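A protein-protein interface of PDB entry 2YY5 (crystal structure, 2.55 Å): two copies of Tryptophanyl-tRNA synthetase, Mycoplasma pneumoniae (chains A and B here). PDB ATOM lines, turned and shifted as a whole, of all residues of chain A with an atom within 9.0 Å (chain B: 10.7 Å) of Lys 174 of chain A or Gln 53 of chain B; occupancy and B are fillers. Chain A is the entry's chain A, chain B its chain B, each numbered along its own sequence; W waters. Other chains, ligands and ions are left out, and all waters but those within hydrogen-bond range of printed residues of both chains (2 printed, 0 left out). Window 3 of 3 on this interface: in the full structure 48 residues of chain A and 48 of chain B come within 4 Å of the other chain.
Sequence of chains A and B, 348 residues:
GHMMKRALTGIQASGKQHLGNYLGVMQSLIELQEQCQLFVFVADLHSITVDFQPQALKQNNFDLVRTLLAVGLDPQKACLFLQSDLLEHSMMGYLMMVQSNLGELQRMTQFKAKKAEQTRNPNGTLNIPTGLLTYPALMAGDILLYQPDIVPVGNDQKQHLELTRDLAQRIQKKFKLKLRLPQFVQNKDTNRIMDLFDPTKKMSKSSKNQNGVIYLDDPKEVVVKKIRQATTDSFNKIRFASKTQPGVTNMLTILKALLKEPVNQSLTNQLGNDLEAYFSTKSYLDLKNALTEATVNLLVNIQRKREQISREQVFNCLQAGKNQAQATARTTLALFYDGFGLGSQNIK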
ATOM      1  N   GLN A  99       9.063  21.325 -22.921  1.00  0.00           N
ATOM      2  CA  GLN A  99       8.571  22.642 -23.295  1.00  0.00           C
ATOM      3  C   GLN A  99       9.268  23.171 -24.552  1.00  0.00           C
ATOM      4  O   GLN A  99       8.888  24.213 -25.077  1.00  0.00           O
ATOM      5  CB  GLN A  99       8.750  23.625 -22.140  1.00  0.00           C
ATOM      6  CG  GLN A  99       7.617  23.600 -21.129  1.00  0.00           C
ATOM      7  CD  GLN A  99       6.285  23.956 -21.751  1.00  0.00           C
ATOM      8  OE1 GLN A  99       5.559  23.091 -22.235  1.00  0.00           O
ATOM      9  NE2 GLN A  99       5.965  25.239 -21.760  1.00  0.00           N
ATOM     10  N   ASP A 166      14.866  31.853 -23.696  1.00  0.00           N
ATOM     11  CA  ASP A 166      13.677  31.592 -24.509  1.00  0.00           C
ATOM     12  C   ASP A 166      12.721  30.654 -23.773  1.00  0.00           C
ATOM     13  O   ASP A 166      11.520  30.908 -23.724  1.00  0.00           O
ATOM     14  CB  ASP A 166      14.037  30.950 -25.856  1.00  0.00           C
ATOM     15  CG  ASP A 166      14.709  31.913 -26.805  1.00  0.00           C
ATOM     16  OD1 ASP A 166      14.534  33.135 -26.626  1.00  0.00           O
ATOM     17  OD2 ASP A 166      15.404  31.441 -27.737  1.00  0.00           O
ATOM     18  N   LEU A 167      13.259  29.563 -23.226  1.00  0.00           N
ATOM     19  CA  LEU A 167      12.456  28.595 -22.486  1.00  0.00           C
ATOM     20  C   LEU A 167      11.906  29.246 -21.226  1.00  0.00           C
ATOM     21  O   LEU A 167      10.751  29.038 -20.854  1.00  0.00           O
ATOM     22  CB  LEU A 167      13.298  27.380 -22.083  1.00  0.00           C
ATOM     23  CG  LEU A 167      13.452  26.131 -22.966  1.00  0.00           C
ATOM     24  CD1 LEU A 167      12.088  25.660 -23.455  1.00  0.00           C
ATOM     25  CD2 LEU A 167      14.344  26.428 -24.123  1.00  0.00           C
ATOM     26  N   ALA A 168      12.741  30.038 -20.569  1.00  0.00           N
ATOM     27  CA  ALA A 168      12.338  30.718 -19.348  1.00  0.00           C
ATOM     28  C   ALA A 168      11.081  31.573 -19.571  1.00  0.00           C
ATOM     29  O   ALA A 168      10.118  31.491 -18.804  1.00  0.00           O
ATOM     30  CB  ALA A 168      13.488  31.579 -18.838  1.00  0.00           C
ATOM     31  N   GLN A 169      11.095  32.378 -20.632  1.00  0.00           N
ATOM     32  CA  GLN A 169       9.970  33.251 -20.959  1.00  0.00           C
ATOM     33  C   GLN A 169       8.761  32.476 -21.429  1.00  0.00           C
ATOM     34  O   GLN A 169       7.621  32.848 -21.143  1.00  0.00           O
ATOM     35  CB  GLN A 169      10.382  34.256 -22.036  1.00  0.00           C
ATOM     36  CG  GLN A 169      11.591  35.071 -21.633  1.00  0.00           C
ATOM     37  CD  GLN A 169      11.836  36.235 -22.549  1.00  0.00           C
ATOM     38  OE1 GLN A 169      11.191  37.283 -22.430  1.00  0.00           O
ATOM     39  NE2 GLN A 169      12.769  36.061 -23.484  1.00  0.00           N
ATOM     40  N   ARG A 170       9.014  31.402 -22.164  1.00  0.00           N
ATOM     41  CA  ARG A 170       7.944  30.562 -22.676  1.00  0.00           C
ATOM     42  C   ARG A 170       7.137  29.966 -21.521  1.00  0.00           C
ATOM     43  O   ARG A 170       5.908  29.982 -21.546  1.00  0.00           O
ATOM     44  CB  ARG A 170       8.537  29.455 -23.550  1.00  0.00           C
ATOM     45  CG  ARG A 170       7.563  28.377 -24.006  1.00  0.00           C
ATOM     46  CD  ARG A 170       8.296  27.386 -24.900  1.00  0.00           C
ATOM     47  NE  ARG A 170       8.998  28.083 -25.977  1.00  0.00           N
ATOM     48  CZ  ARG A 170       9.861  27.526 -26.827  1.00  0.00           C
ATOM     49  NH1 ARG A 170      10.169  26.233 -26.766  1.00  0.00           N
ATOM     50  NH2 ARG A 170      10.431  28.284 -27.743  1.00  0.00           N
ATOM     51  N   ILE A 171       7.836  29.464 -20.506  1.00  0.00           N
ATOM     52  CA  ILE A 171       7.191  28.852 -19.339  1.00  0.00           C
ATOM     53  C   ILE A 171       6.549  29.910 -18.443  1.00  0.00           C
ATOM     54  O   ILE A 171       5.512  29.683 -17.810  1.00  0.00           O
ATOM     55  CB  ILE A 171       8.221  28.048 -18.522  1.00  0.00           C
ATOM     56  CG1 ILE A 171       8.837  26.959 -19.404  1.00  0.00           C
ATOM     57  CG2 ILE A 171       7.557  27.412 -17.319  1.00  0.00           C
ATOM     58  CD1 ILE A 171      10.082  26.345 -18.830  1.00  0.00           C
ATOM     59  N   GLN A 172       7.178  31.073 -18.410  1.00  0.00           N
ATOM     60  CA  GLN A 172       6.713  32.204 -17.624  1.00  0.00           C
ATOM     61  C   GLN A 172       5.368  32.681 -18.147  1.00  0.00           C
ATOM     62  O   GLN A 172       4.496  33.090 -17.379  1.00  0.00           O
ATOM     63  CB  GLN A 172       7.755  33.318 -17.711  1.00  0.00           C
ATOM     64  CG  GLN A 172       7.356  34.652 -17.150  1.00  0.00           C
ATOM     65  CD  GLN A 172       8.513  35.637 -17.185  1.00  0.00           C
ATOM     66  OE1 GLN A 172       9.119  35.941 -16.151  1.00  0.00           O
ATOM     67  NE2 GLN A 172       8.838  36.130 -18.382  1.00  0.00           N
ATOM     68  N   LYS A 173       5.201  32.617 -19.461  1.00  0.00           N
ATOM     69  CA  LYS A 173       3.956  33.039 -20.084  1.00  0.00           C
ATOM     70  C   LYS A 173       2.909  31.927 -20.039  1.00  0.00           C
ATOM     71  O   LYS A 173       1.737  32.183 -19.794  1.00  0.00           O
ATOM     72  CB  LYS A 173       4.209  33.444 -21.529  1.00  0.00           C
ATOM     73  CG  LYS A 173       3.014  34.069 -22.190  1.00  0.00           C
ATOM     74  CD  LYS A 173       3.300  34.407 -23.630  1.00  0.00           C
ATOM     75  CE  LYS A 173       2.156  35.206 -24.215  1.00  0.00           C
ATOM     76  NZ  LYS A 173       2.478  35.614 -25.604  1.00  0.00           N
ATOM     77  N   LYS A 174       3.339  30.691 -20.270  1.00  0.00           N
ATOM     78  CA  LYS A 174       2.434  29.537 -20.263  1.00  0.00           C
ATOM     79  C   LYS A 174       1.876  29.214 -18.876  1.00  0.00           C
ATOM     80  O   LYS A 174       0.684  28.964 -18.719  1.00  0.00           O
ATOM     81  CB  LYS A 174       3.171  28.304 -20.806  1.00  0.00           C
ATOM     82  CG  LYS A 174       2.277  27.220 -21.400  1.00  0.00           C
ATOM     83  CD  LYS A 174       1.598  26.370 -20.355  1.00  0.00           C
ATOM     84  CE  LYS A 174       0.662  25.348 -21.001  1.00  0.00           C
ATOM     85  NZ  LYS A 174      -0.556  25.971 -21.610  1.00  0.00           N
ATOM     86  N   PHE A 175       2.734  29.237 -17.863  1.00  0.00           N
ATOM     87  CA  PHE A 175       2.303  28.889 -16.519  1.00  0.00           C
ATOM     88  C   PHE A 175       2.148  30.006 -15.495  1.00  0.00           C
ATOM     89  O   PHE A 175       1.747  29.741 -14.360  1.00  0.00           O
ATOM     90  CB  PHE A 175       3.247  27.834 -15.955  1.00  0.00           C
ATOM     91  CG  PHE A 175       3.399  26.633 -16.836  1.00  0.00           C
ATOM     92  CD1 PHE A 175       4.342  26.615 -17.853  1.00  0.00           C
ATOM     93  CD2 PHE A 175       2.605  25.511 -16.642  1.00  0.00           C
ATOM     94  CE1 PHE A 175       4.500  25.492 -18.663  1.00  0.00           C
ATOM     95  CE2 PHE A 175       2.754  24.385 -17.448  1.00  0.00           C
ATOM     96  CZ  PHE A 175       3.707  24.378 -18.461  1.00  0.00           C
ATOM     97  N   LYS A 176       2.457  31.242 -15.878  1.00  0.00           N
ATOM     98  CA  LYS A 176       2.353  32.382 -14.963  1.00  0.00           C
ATOM     99  C   LYS A 176       3.347  32.224 -13.820  1.00  0.00           C
ATOM    100  O   LYS A 176       3.152  32.773 -12.741  1.00  0.00           O
ATOM    101  CB  LYS A 176       0.944  32.490 -14.363  1.00  0.00           C
ATOM    102  CG  LYS A 176      -0.226  32.427 -15.355  1.00  0.00           C
ATOM    103  CD  LYS A 176      -0.347  33.661 -16.248  1.00  0.00           C
ATOM    104  CE  LYS A 176       0.622  33.613 -17.417  1.00  0.00           C
ATOM    105  NZ  LYS A 176       0.371  34.698 -18.410  1.00  0.00           N
ATOM    106  N   LEU A 177       4.408  31.468 -14.066  1.00  0.00           N
ATOM    107  CA  LEU A 177       5.443  31.214 -13.069  1.00  0.00           C
ATOM    108  C   LEU A 177       6.306  32.444 -12.783  1.00  0.00           C
ATOM    109  O   LEU A 177       6.715  33.157 -13.699  1.00  0.00           O
ATOM    110  CB  LEU A 177       6.333  30.066 -13.555  1.00  0.00           C
ATOM    111  CG  LEU A 177       6.485  28.845 -12.653  1.00  0.00           C
ATOM    112  CD1 LEU A 177       5.155  28.494 -12.014  1.00  0.00           C
ATOM    113  CD2 LEU A 177       7.007  27.689 -13.482  1.00  0.00           C
ATOM    114  N   LEU A 179       9.406  34.023 -12.520  1.00  0.00           N
ATOM    115  CA  LEU A 179      10.753  33.671 -12.953  1.00  0.00           C
ATOM    116  C   LEU A 179      11.725  34.826 -13.003  1.00  0.00           C
ATOM    117  O   LEU A 179      11.339  35.989 -13.100  1.00  0.00           O
ATOM    118  CB  LEU A 179      10.706  33.031 -14.344  1.00  0.00           C
ATOM    119  CG  LEU A 179      10.933  31.528 -14.435  1.00  0.00           C
ATOM    120  CD1 LEU A 179      10.080  30.800 -13.411  1.00  0.00           C
ATOM    121  CD2 LEU A 179      10.602  31.070 -15.836  1.00  0.00           C
ATOM    122  N   GLY A 339       3.264  24.792 -10.626  1.00  0.00           N
ATOM    123  CA  GLY A 339       2.958  25.570 -11.808  1.00  0.00           C
ATOM    124  C   GLY A 339       2.574  24.665 -12.968  1.00  0.00           C
ATOM    125  O   GLY A 339       1.733  25.032 -13.798  1.00  0.00           O
ATOM    126  N   PHE A 340       3.201  23.486 -13.037  1.00  0.00           N
ATOM    127  CA  PHE A 340       2.914  22.518 -14.095  1.00  0.00           C
ATOM    128  C   PHE A 340       1.797  21.584 -13.647  1.00  0.00           C
ATOM    129  O   PHE A 340       1.322  20.762 -14.432  1.00  0.00           O
ATOM    130  CB  PHE A 340       4.142  21.658 -14.417  1.00  0.00           C
ATOM    131  CG  PHE A 340       5.143  22.313 -15.330  1.00  0.00           C
ATOM    132  CD1 PHE A 340       5.717  23.541 -15.008  1.00  0.00           C
ATOM    133  CD2 PHE A 340       5.559  21.665 -16.496  1.00  0.00           C
ATOM    134  CE1 PHE A 340       6.691  24.110 -15.830  1.00  0.00           C
ATOM    135  CE2 PHE A 340       6.529  22.226 -17.322  1.00  0.00           C
ATOM    136  CZ  PHE A 340       7.095  23.455 -16.984  1.00  0.00           C
ATOM    137  N   GLY A 341       1.398  21.690 -12.382  1.00  0.00           N
ATOM    138  CA  GLY A 341       0.341  20.830 -11.877  1.00  0.00           C
ATOM    139  C   GLY A 341       0.798  19.395 -11.688  1.00  0.00           C
ATOM    140  O   GLY A 341       0.006  18.457 -11.773  1.00  0.00           O
ATOM    141  N   LEU A 342       2.089  19.224 -11.435  1.00  0.00           N
ATOM    142  CA  LEU A 342       2.677  17.911 -11.217  1.00  0.00           C
ATOM    143  C   LEU A 342       2.715  17.582  -9.731  1.00  0.00           C
ATOM    144  O   LEU A 342       2.551  18.465  -8.900  1.00  0.00           O
ATOM    145  CB  LEU A 342       4.102  17.892 -11.759  1.00  0.00           C
ATOM    146  CG  LEU A 342       4.407  17.392 -13.175  1.00  0.00           C
ATOM    147  CD1 LEU A 342       3.140  17.103 -13.921  1.00  0.00           C
ATOM    148  CD2 LEU A 342       5.261  18.419 -13.895  1.00  0.00           C
ATOM    149  N   ALA B  13      -3.319   9.740 -17.715  1.00  0.00           N
ATOM    150  CA  ALA B  13      -4.629  10.237 -17.310  1.00  0.00           C
ATOM    151  C   ALA B  13      -5.205  11.092 -18.435  1.00  0.00           C
ATOM    152  O   ALA B  13      -4.461  11.694 -19.212  1.00  0.00           O
ATOM    153  CB  ALA B  13      -4.520  11.051 -16.018  1.00  0.00           C
ATOM    154  N   SER B  14      -6.533  11.142 -18.507  1.00  0.00           N
ATOM    155  CA  SER B  14      -7.221  11.901 -19.534  1.00  0.00           C
ATOM    156  C   SER B  14      -8.732  11.756 -19.403  1.00  0.00           C
ATOM    157  O   SER B  14      -9.246  10.657 -19.163  1.00  0.00           O
ATOM    158  CB  SER B  14      -6.791  11.408 -20.919  1.00  0.00           C
ATOM    159  OG  SER B  14      -7.637  11.923 -21.927  1.00  0.00           O
ATOM    160  N   GLY B  15      -9.444  12.866 -19.573  1.00  0.00           N
ATOM    161  CA  GLY B  15     -10.892  12.827 -19.491  1.00  0.00           C
ATOM    162  C   GLY B  15     -11.406  11.974 -20.625  1.00  0.00           C
ATOM    163  O   GLY B  15     -12.602  11.738 -20.757  1.00  0.00           O
ATOM    164  N   ASP B  44       1.905  10.817 -15.639  1.00  0.00           N
ATOM    165  CA  ASP B  44       1.754  12.245 -15.917  1.00  0.00           C
ATOM    166  C   ASP B  44       2.972  12.923 -16.547  1.00  0.00           C
ATOM    167  O   ASP B  44       2.898  14.082 -16.946  1.00  0.00           O
ATOM    168  CB  ASP B  44       1.356  12.996 -14.644  1.00  0.00           C
ATOM    169  CG  ASP B  44       2.349  12.801 -13.507  1.00  0.00           C
ATOM    170  OD1 ASP B  44       2.349  13.648 -12.591  1.00  0.00           O
ATOM    171  OD2 ASP B  44       3.113  11.806 -13.515  1.00  0.00           O
ATOM    172  N   SER B  47       2.112  12.693 -20.192  1.00  0.00           N
ATOM    173  CA  SER B  47       1.014  13.577 -20.565  1.00  0.00           C
ATOM    174  C   SER B  47       1.490  14.973 -20.955  1.00  0.00           C
ATOM    175  O   SER B  47       0.965  15.573 -21.897  1.00  0.00           O
ATOM    176  CB  SER B  47       0.016  13.679 -19.411  1.00  0.00           C
ATOM    177  OG  SER B  47      -0.535  12.414 -19.138  1.00  0.00           O
ATOM    178  N   ILE B  48       2.483  15.484 -20.232  1.00  0.00           N
ATOM    179  CA  ILE B  48       3.012  16.811 -20.516  1.00  0.00           C
ATOM    180  C   ILE B  48       3.996  16.845 -21.689  1.00  0.00           C
ATOM    181  O   ILE B  48       4.758  17.798 -21.824  1.00  0.00           O
ATOM    182  CB  ILE B  48       3.708  17.424 -19.283  1.00  0.00           C
ATOM    183  CG1 ILE B  48       4.936  16.599 -18.899  1.00  0.00           C
ATOM    184  CG2 ILE B  48       2.742  17.495 -18.114  1.00  0.00           C
ATOM    185  CD1 ILE B  48       5.822  17.309 -17.890  1.00  0.00           C
ATOM    186  N   THR B  49       4.003  15.809 -22.524  1.00  0.00           N
ATOM    187  CA  THR B  49       4.896  15.816 -23.675  1.00  0.00           C
ATOM    188  C   THR B  49       4.248  16.627 -24.795  1.00  0.00           C
ATOM    189  O   THR B  49       4.861  16.875 -25.828  1.00  0.00           O
ATOM    190  CB  THR B  49       5.251  14.384 -24.179  1.00  0.00           C
ATOM    191  OG1 THR B  49       4.062  13.616 -24.385  1.00  0.00           O
ATOM    192  CG2 THR B  49       6.154  13.680 -23.175  1.00  0.00           C
ATOM    193  N   VAL B  50       2.999  17.034 -24.579  1.00  0.00           N
ATOM    194  CA  VAL B  50       2.270  17.872 -25.534  1.00  0.00           C
ATOM    195  C   VAL B  50       1.644  19.015 -24.733  1.00  0.00           C
ATOM    196  O   VAL B  50       1.539  18.928 -23.509  1.00  0.00           O
ATOM    197  CB  VAL B  50       1.132  17.097 -26.291  1.00  0.00           C
ATOM    198  CG1 VAL B  50       1.728  16.126 -27.296  1.00  0.00           C
ATOM    199  CG2 VAL B  50       0.246  16.355 -25.307  1.00  0.00           C
ATOM    200  N   ASP B  51       1.245  20.089 -25.412  1.00  0.00           N
ATOM    201  CA  ASP B  51       0.629  21.221 -24.730  1.00  0.00           C
ATOM    202  C   ASP B  51      -0.477  20.680 -23.828  1.00  0.00           C
ATOM    203  O   ASP B  51      -1.211  19.768 -24.212  1.00  0.00           O
ATOM    204  CB  ASP B  51       0.054  22.210 -25.747  1.00  0.00           C
ATOM    205  CG  ASP B  51      -0.510  23.455 -25.092  1.00  0.00           C
ATOM    206  OD1 ASP B  51       0.203  24.087 -24.282  1.00  0.00           O
ATOM    207  OD2 ASP B  51      -1.669  23.805 -25.391  1.00  0.00           O
ATOM    208  N   PHE B  52      -0.592  21.238 -22.630  1.00  0.00           N
ATOM    209  CA  PHE B  52      -1.589  20.760 -21.680  1.00  0.00           C
ATOM    210  C   PHE B  52      -1.919  21.858 -20.669  1.00  0.00           C
ATOM    211  O   PHE B  52      -1.161  22.807 -20.504  1.00  0.00           O
ATOM    212  CB  PHE B  52      -1.015  19.556 -20.930  1.00  0.00           C
ATOM    213  CG  PHE B  52      -0.011  19.943 -19.884  1.00  0.00           C
ATOM    214  CD1 PHE B  52      -0.411  20.164 -18.566  1.00  0.00           C
ATOM    215  CD2 PHE B  52       1.312  20.197 -20.233  1.00  0.00           C
ATOM    216  CE1 PHE B  52       0.489  20.640 -17.612  1.00  0.00           C
ATOM    217  CE2 PHE B  52       2.222  20.677 -19.284  1.00  0.00           C
ATOM    218  CZ  PHE B  52       1.806  20.900 -17.971  1.00  0.00           C
ATOM    219  N   GLN B  53      -3.040  21.721 -19.977  1.00  0.00           N
ATOM    220  CA  GLN B  53      -3.416  22.713 -18.975  1.00  0.00           C
ATOM    221  C   GLN B  53      -3.183  22.152 -17.572  1.00  0.00           C
ATOM    222  O   GLN B  53      -3.798  21.164 -17.174  1.00  0.00           O
ATOM    223  CB  GLN B  53      -4.888  23.119 -19.138  1.00  0.00           C
ATOM    224  CG  GLN B  53      -5.219  23.827 -20.452  1.00  0.00           C
ATOM    225  CD  GLN B  53      -4.458  25.134 -20.634  1.00  0.00           C
ATOM    226  OE1 GLN B  53      -4.480  26.011 -19.762  1.00  0.00           O
ATOM    227  NE2 GLN B  53      -3.787  25.273 -21.777  1.00  0.00           N
ATOM    228  N   PRO B  54      -2.282  22.775 -16.805  1.00  0.00           N
ATOM    229  CA  PRO B  54      -1.989  22.310 -15.445  1.00  0.00           C
ATOM    230  C   PRO B  54      -3.224  22.029 -14.584  1.00  0.00           C
ATOM    231  O   PRO B  54      -3.198  21.175 -13.699  1.00  0.00           O
ATOM    232  CB  PRO B  54      -1.094  23.424 -14.877  1.00  0.00           C
ATOM    233  CG  PRO B  54      -1.350  24.602 -15.781  1.00  0.00           C
ATOM    234  CD  PRO B  54      -1.493  23.973 -17.130  1.00  0.00           C
ATOM    235  N   GLN B  55      -4.306  22.745 -14.853  1.00  0.00           N
ATOM    236  CA  GLN B  55      -5.542  22.559 -14.108  1.00  0.00           C
ATOM    237  C   GLN B  55      -6.153  21.228 -14.517  1.00  0.00           C
ATOM    238  O   GLN B  55      -6.609  20.445 -13.680  1.00  0.00           O
ATOM    239  CB  GLN B  55      -6.520  23.688 -14.432  1.00  0.00           C
ATOM    240  CG  GLN B  55      -6.039  25.079 -14.049  1.00  0.00           C
ATOM    241  CD  GLN B  55      -6.378  25.434 -12.614  1.00  0.00           C
ATOM    242  OE1 GLN B  55      -6.019  24.710 -11.677  1.00  0.00           O
ATOM    243  NE2 GLN B  55      -7.077  26.556 -12.433  1.00  0.00           N
ATOM    244  N   ALA B  56      -6.158  20.987 -15.822  1.00  0.00           N
ATOM    245  CA  ALA B  56      -6.708  19.765 -16.389  1.00  0.00           C
ATOM    246  C   ALA B  56      -5.889  18.552 -15.969  1.00  0.00           C
ATOM    247  O   ALA B  56      -6.446  17.500 -15.672  1.00  0.00           O
ATOM    248  CB  ALA B  56      -6.743  19.870 -17.912  1.00  0.00           C
ATOM    249  N   LEU B  57      -4.567  18.709 -15.947  1.00  0.00           N
ATOM    250  CA  LEU B  57      -3.665  17.626 -15.573  1.00  0.00           C
ATOM    251  C   LEU B  57      -4.004  17.178 -14.150  1.00  0.00           C
ATOM    252  O   LEU B  57      -4.239  15.999 -13.899  1.00  0.00           O
ATOM    253  CB  LEU B  57      -2.207  18.114 -15.676  1.00  0.00           C
ATOM    254  CG  LEU B  57      -0.994  17.163 -15.741  1.00  0.00           C
ATOM    255  CD1 LEU B  57      -0.164  17.335 -14.490  1.00  0.00           C
ATOM    256  CD2 LEU B  57      -1.422  15.707 -15.901  1.00  0.00           C
ATOM    257  N   LYS B  58      -4.051  18.131 -13.227  1.00  0.00           N
ATOM    258  CA  LYS B  58      -4.366  17.836 -11.832  1.00  0.00           C
ATOM    259  C   LYS B  58      -5.695  17.106 -11.702  1.00  0.00           C
ATOM    260  O   LYS B  58      -5.785  16.073 -11.035  1.00  0.00           O
ATOM    261  CB  LYS B  58      -4.412  19.132 -11.018  1.00  0.00           C
ATOM    262  CG  LYS B  58      -3.114  19.448 -10.295  1.00  0.00           C
ATOM    263  CD  LYS B  58      -2.872  20.950 -10.174  1.00  0.00           C
ATOM    264  CE  LYS B  58      -3.979  21.666  -9.420  1.00  0.00           C
ATOM    265  NZ  LYS B  58      -3.702  23.125  -9.363  1.00  0.00           N
ATOM    266  N   GLN B  59      -6.724  17.641 -12.347  1.00  0.00           N
ATOM    267  CA  GLN B  59      -8.044  17.039 -12.283  1.00  0.00           C
ATOM    268  C   GLN B  59      -8.035  15.607 -12.812  1.00  0.00           C
ATOM    269  O   GLN B  59      -8.610  14.705 -12.194  1.00  0.00           O
ATOM    270  CB  GLN B  59      -9.048  17.891 -13.067  1.00  0.00           C
ATOM    271  CG  GLN B  59     -10.483  17.352 -13.068  1.00  0.00           C
ATOM    272  CD  GLN B  59     -10.973  16.947 -11.681  1.00  0.00           C
ATOM    273  OE1 GLN B  59     -10.694  17.618 -10.688  1.00  0.00           O
ATOM    274  NE2 GLN B  59     -11.714  15.848 -11.614  1.00  0.00           N
ATOM    275  N   ASN B  60      -7.361  15.402 -13.942  1.00  0.00           N
ATOM    276  CA  ASN B  60      -7.271  14.088 -14.567  1.00  0.00           C
ATOM    277  C   ASN B  60      -6.488  13.068 -13.735  1.00  0.00           C
ATOM    278  O   ASN B  60      -6.939  11.930 -13.580  1.00  0.00           O
ATOM    279  CB  ASN B  60      -6.660  14.216 -15.964  1.00  0.00           C
ATOM    280  CG  ASN B  60      -7.623  14.822 -16.973  1.00  0.00           C
ATOM    281  OD1 ASN B  60      -7.242  15.109 -18.113  1.00  0.00           O
ATOM    282  ND2 ASN B  60      -8.881  15.009 -16.567  1.00  0.00           N
ATOM    283  N   ASN B  61      -5.323  13.463 -13.213  1.00  0.00           N
ATOM    284  CA  ASN B  61      -4.524  12.558 -12.380  1.00  0.00           C
ATOM    285  C   ASN B  61      -5.400  12.053 -11.230  1.00  0.00           C
ATOM    286  O   ASN B  61      -5.385  10.872 -10.883  1.00  0.00           O
ATOM    287  CB  ASN B  61      -3.283  13.265 -11.810  1.00  0.00           C
ATOM    288  CG  ASN B  61      -2.240  13.580 -12.874  1.00  0.00           C
ATOM    289  OD1 ASN B  61      -2.304  13.071 -13.994  1.00  0.00           O
ATOM    290  ND2 ASN B  61      -1.266  14.417 -12.521  1.00  0.00           N
HETATM  291  O   HOH W   1       3.246  23.325 -24.435  1.00  0.00           O
HETATM  292  O   HOH W   2      -0.931  16.309 -10.106  1.00  0.00           O
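NZ of Lys 174 of chain A lies within salt-bridge range of OD1 of Asp 51 of chain B (3.4 Å). NZ of Lys 174 of chain A sits close to O of Phe 52 of chain B, 3.4 Å away. The side-chain amino group of Lys 174 of chain A sits close to the side-chain amide nitrogen of Gln 53 of chain B (3.3 Å).
Phe 175 of chain A touches Phe 52 of chain B (CE2 to CZ, 3.6 Å). O of Gly 339 of chain A touches CB of Pro 54 of chain B, 3.4 Å away. Phe 340 of chain A touches Phe 52 of chain B. Pro 54 of chain B touches Phe 340 of chain A. Phe 340 of chain A touches Leu 57 of chain B. CB of Pro 54 of chain B touches N of Gly 341 of chain A, 3.9 Å away. O of Gly 341 of chain A touches CD1 of Leu 57 of chain B, at 2.9 Å. Lys 58 of chain B touches Gly 341 of chain A. Asp 44 of chain B touches Leu 342 of chain A (OD1 to CD1, 3.8 Å). CD1 of Leu 342 of chain A touches CD1 of Leu 57 of chain B, 3.4 Å away.
Of chain B, only Asp 51, Phe 52 and Gln 53 come within 4 Å of Lys 174 of chain A. Phe 175 of chain A touches just one residue of chain B: Phe 52. Leu 179 of chain A touches none of the printed residues of chain B. Printed residues of chain B within 4 Å of Gly 341 of chain A: Pro 54, Leu 57 and Lys 58. Of the printed residues of chain B, Leu 342 of chain A touches Asp 44 and Leu 57. Printed residues of chain A within 4 Å of Gln 53 of chain B: Lys 174 (3.3 Å). Of the printed residues of chain A, Pro 54 of chain B touches Gly 339 (3.4 Å), Phe 340 (3.6 Å) and Gly 341 (3.9 Å). No residue of chain A comes within 4 Å of Ala 56 of chain B. The nearest residue of chain B that does not touch Lys 174 of chain A is Pro 54 of chain B (4.6 Å). The nearest residue of chain A that does not touch Gln 53 of chain B is Phe 340 of chain A (5.7 Å).
Printed residues of chain B that touch a printed residue of chain A: Asp 44, Asp 51, Phe 52, Gln 53, Pro 54, Leu 57 and Lys 58. Hydrophobic or aromatic side chains of chain B within 4 Å of the printed part of chain A: Phe 52, Pro 54 and Leu 57. Printed residues of chain A that touch a printed residue of chain B: Lys 174, Phe 175, Gly 339, Phe 340, Gly 341 and Leu 342. Hydrophobic or aromatic side chains of chain A within 4 Å of the printed part of chain B: Phe 175 and Leu 342. Among the printed residues, 13 pairs touch across the chains.
No position is printed for both chains.
Water W2 lies within hydrogen-bond range of the backbone carbonyl oxygen of Gly 341 of chain A (2.9 Å) and the side-chain amide nitrogen of Asn 61 of chain B (3.1 Å). Water W1 bridges OD1 of Asp 51 of chain B and OE1 of Gln 99 of chain A.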
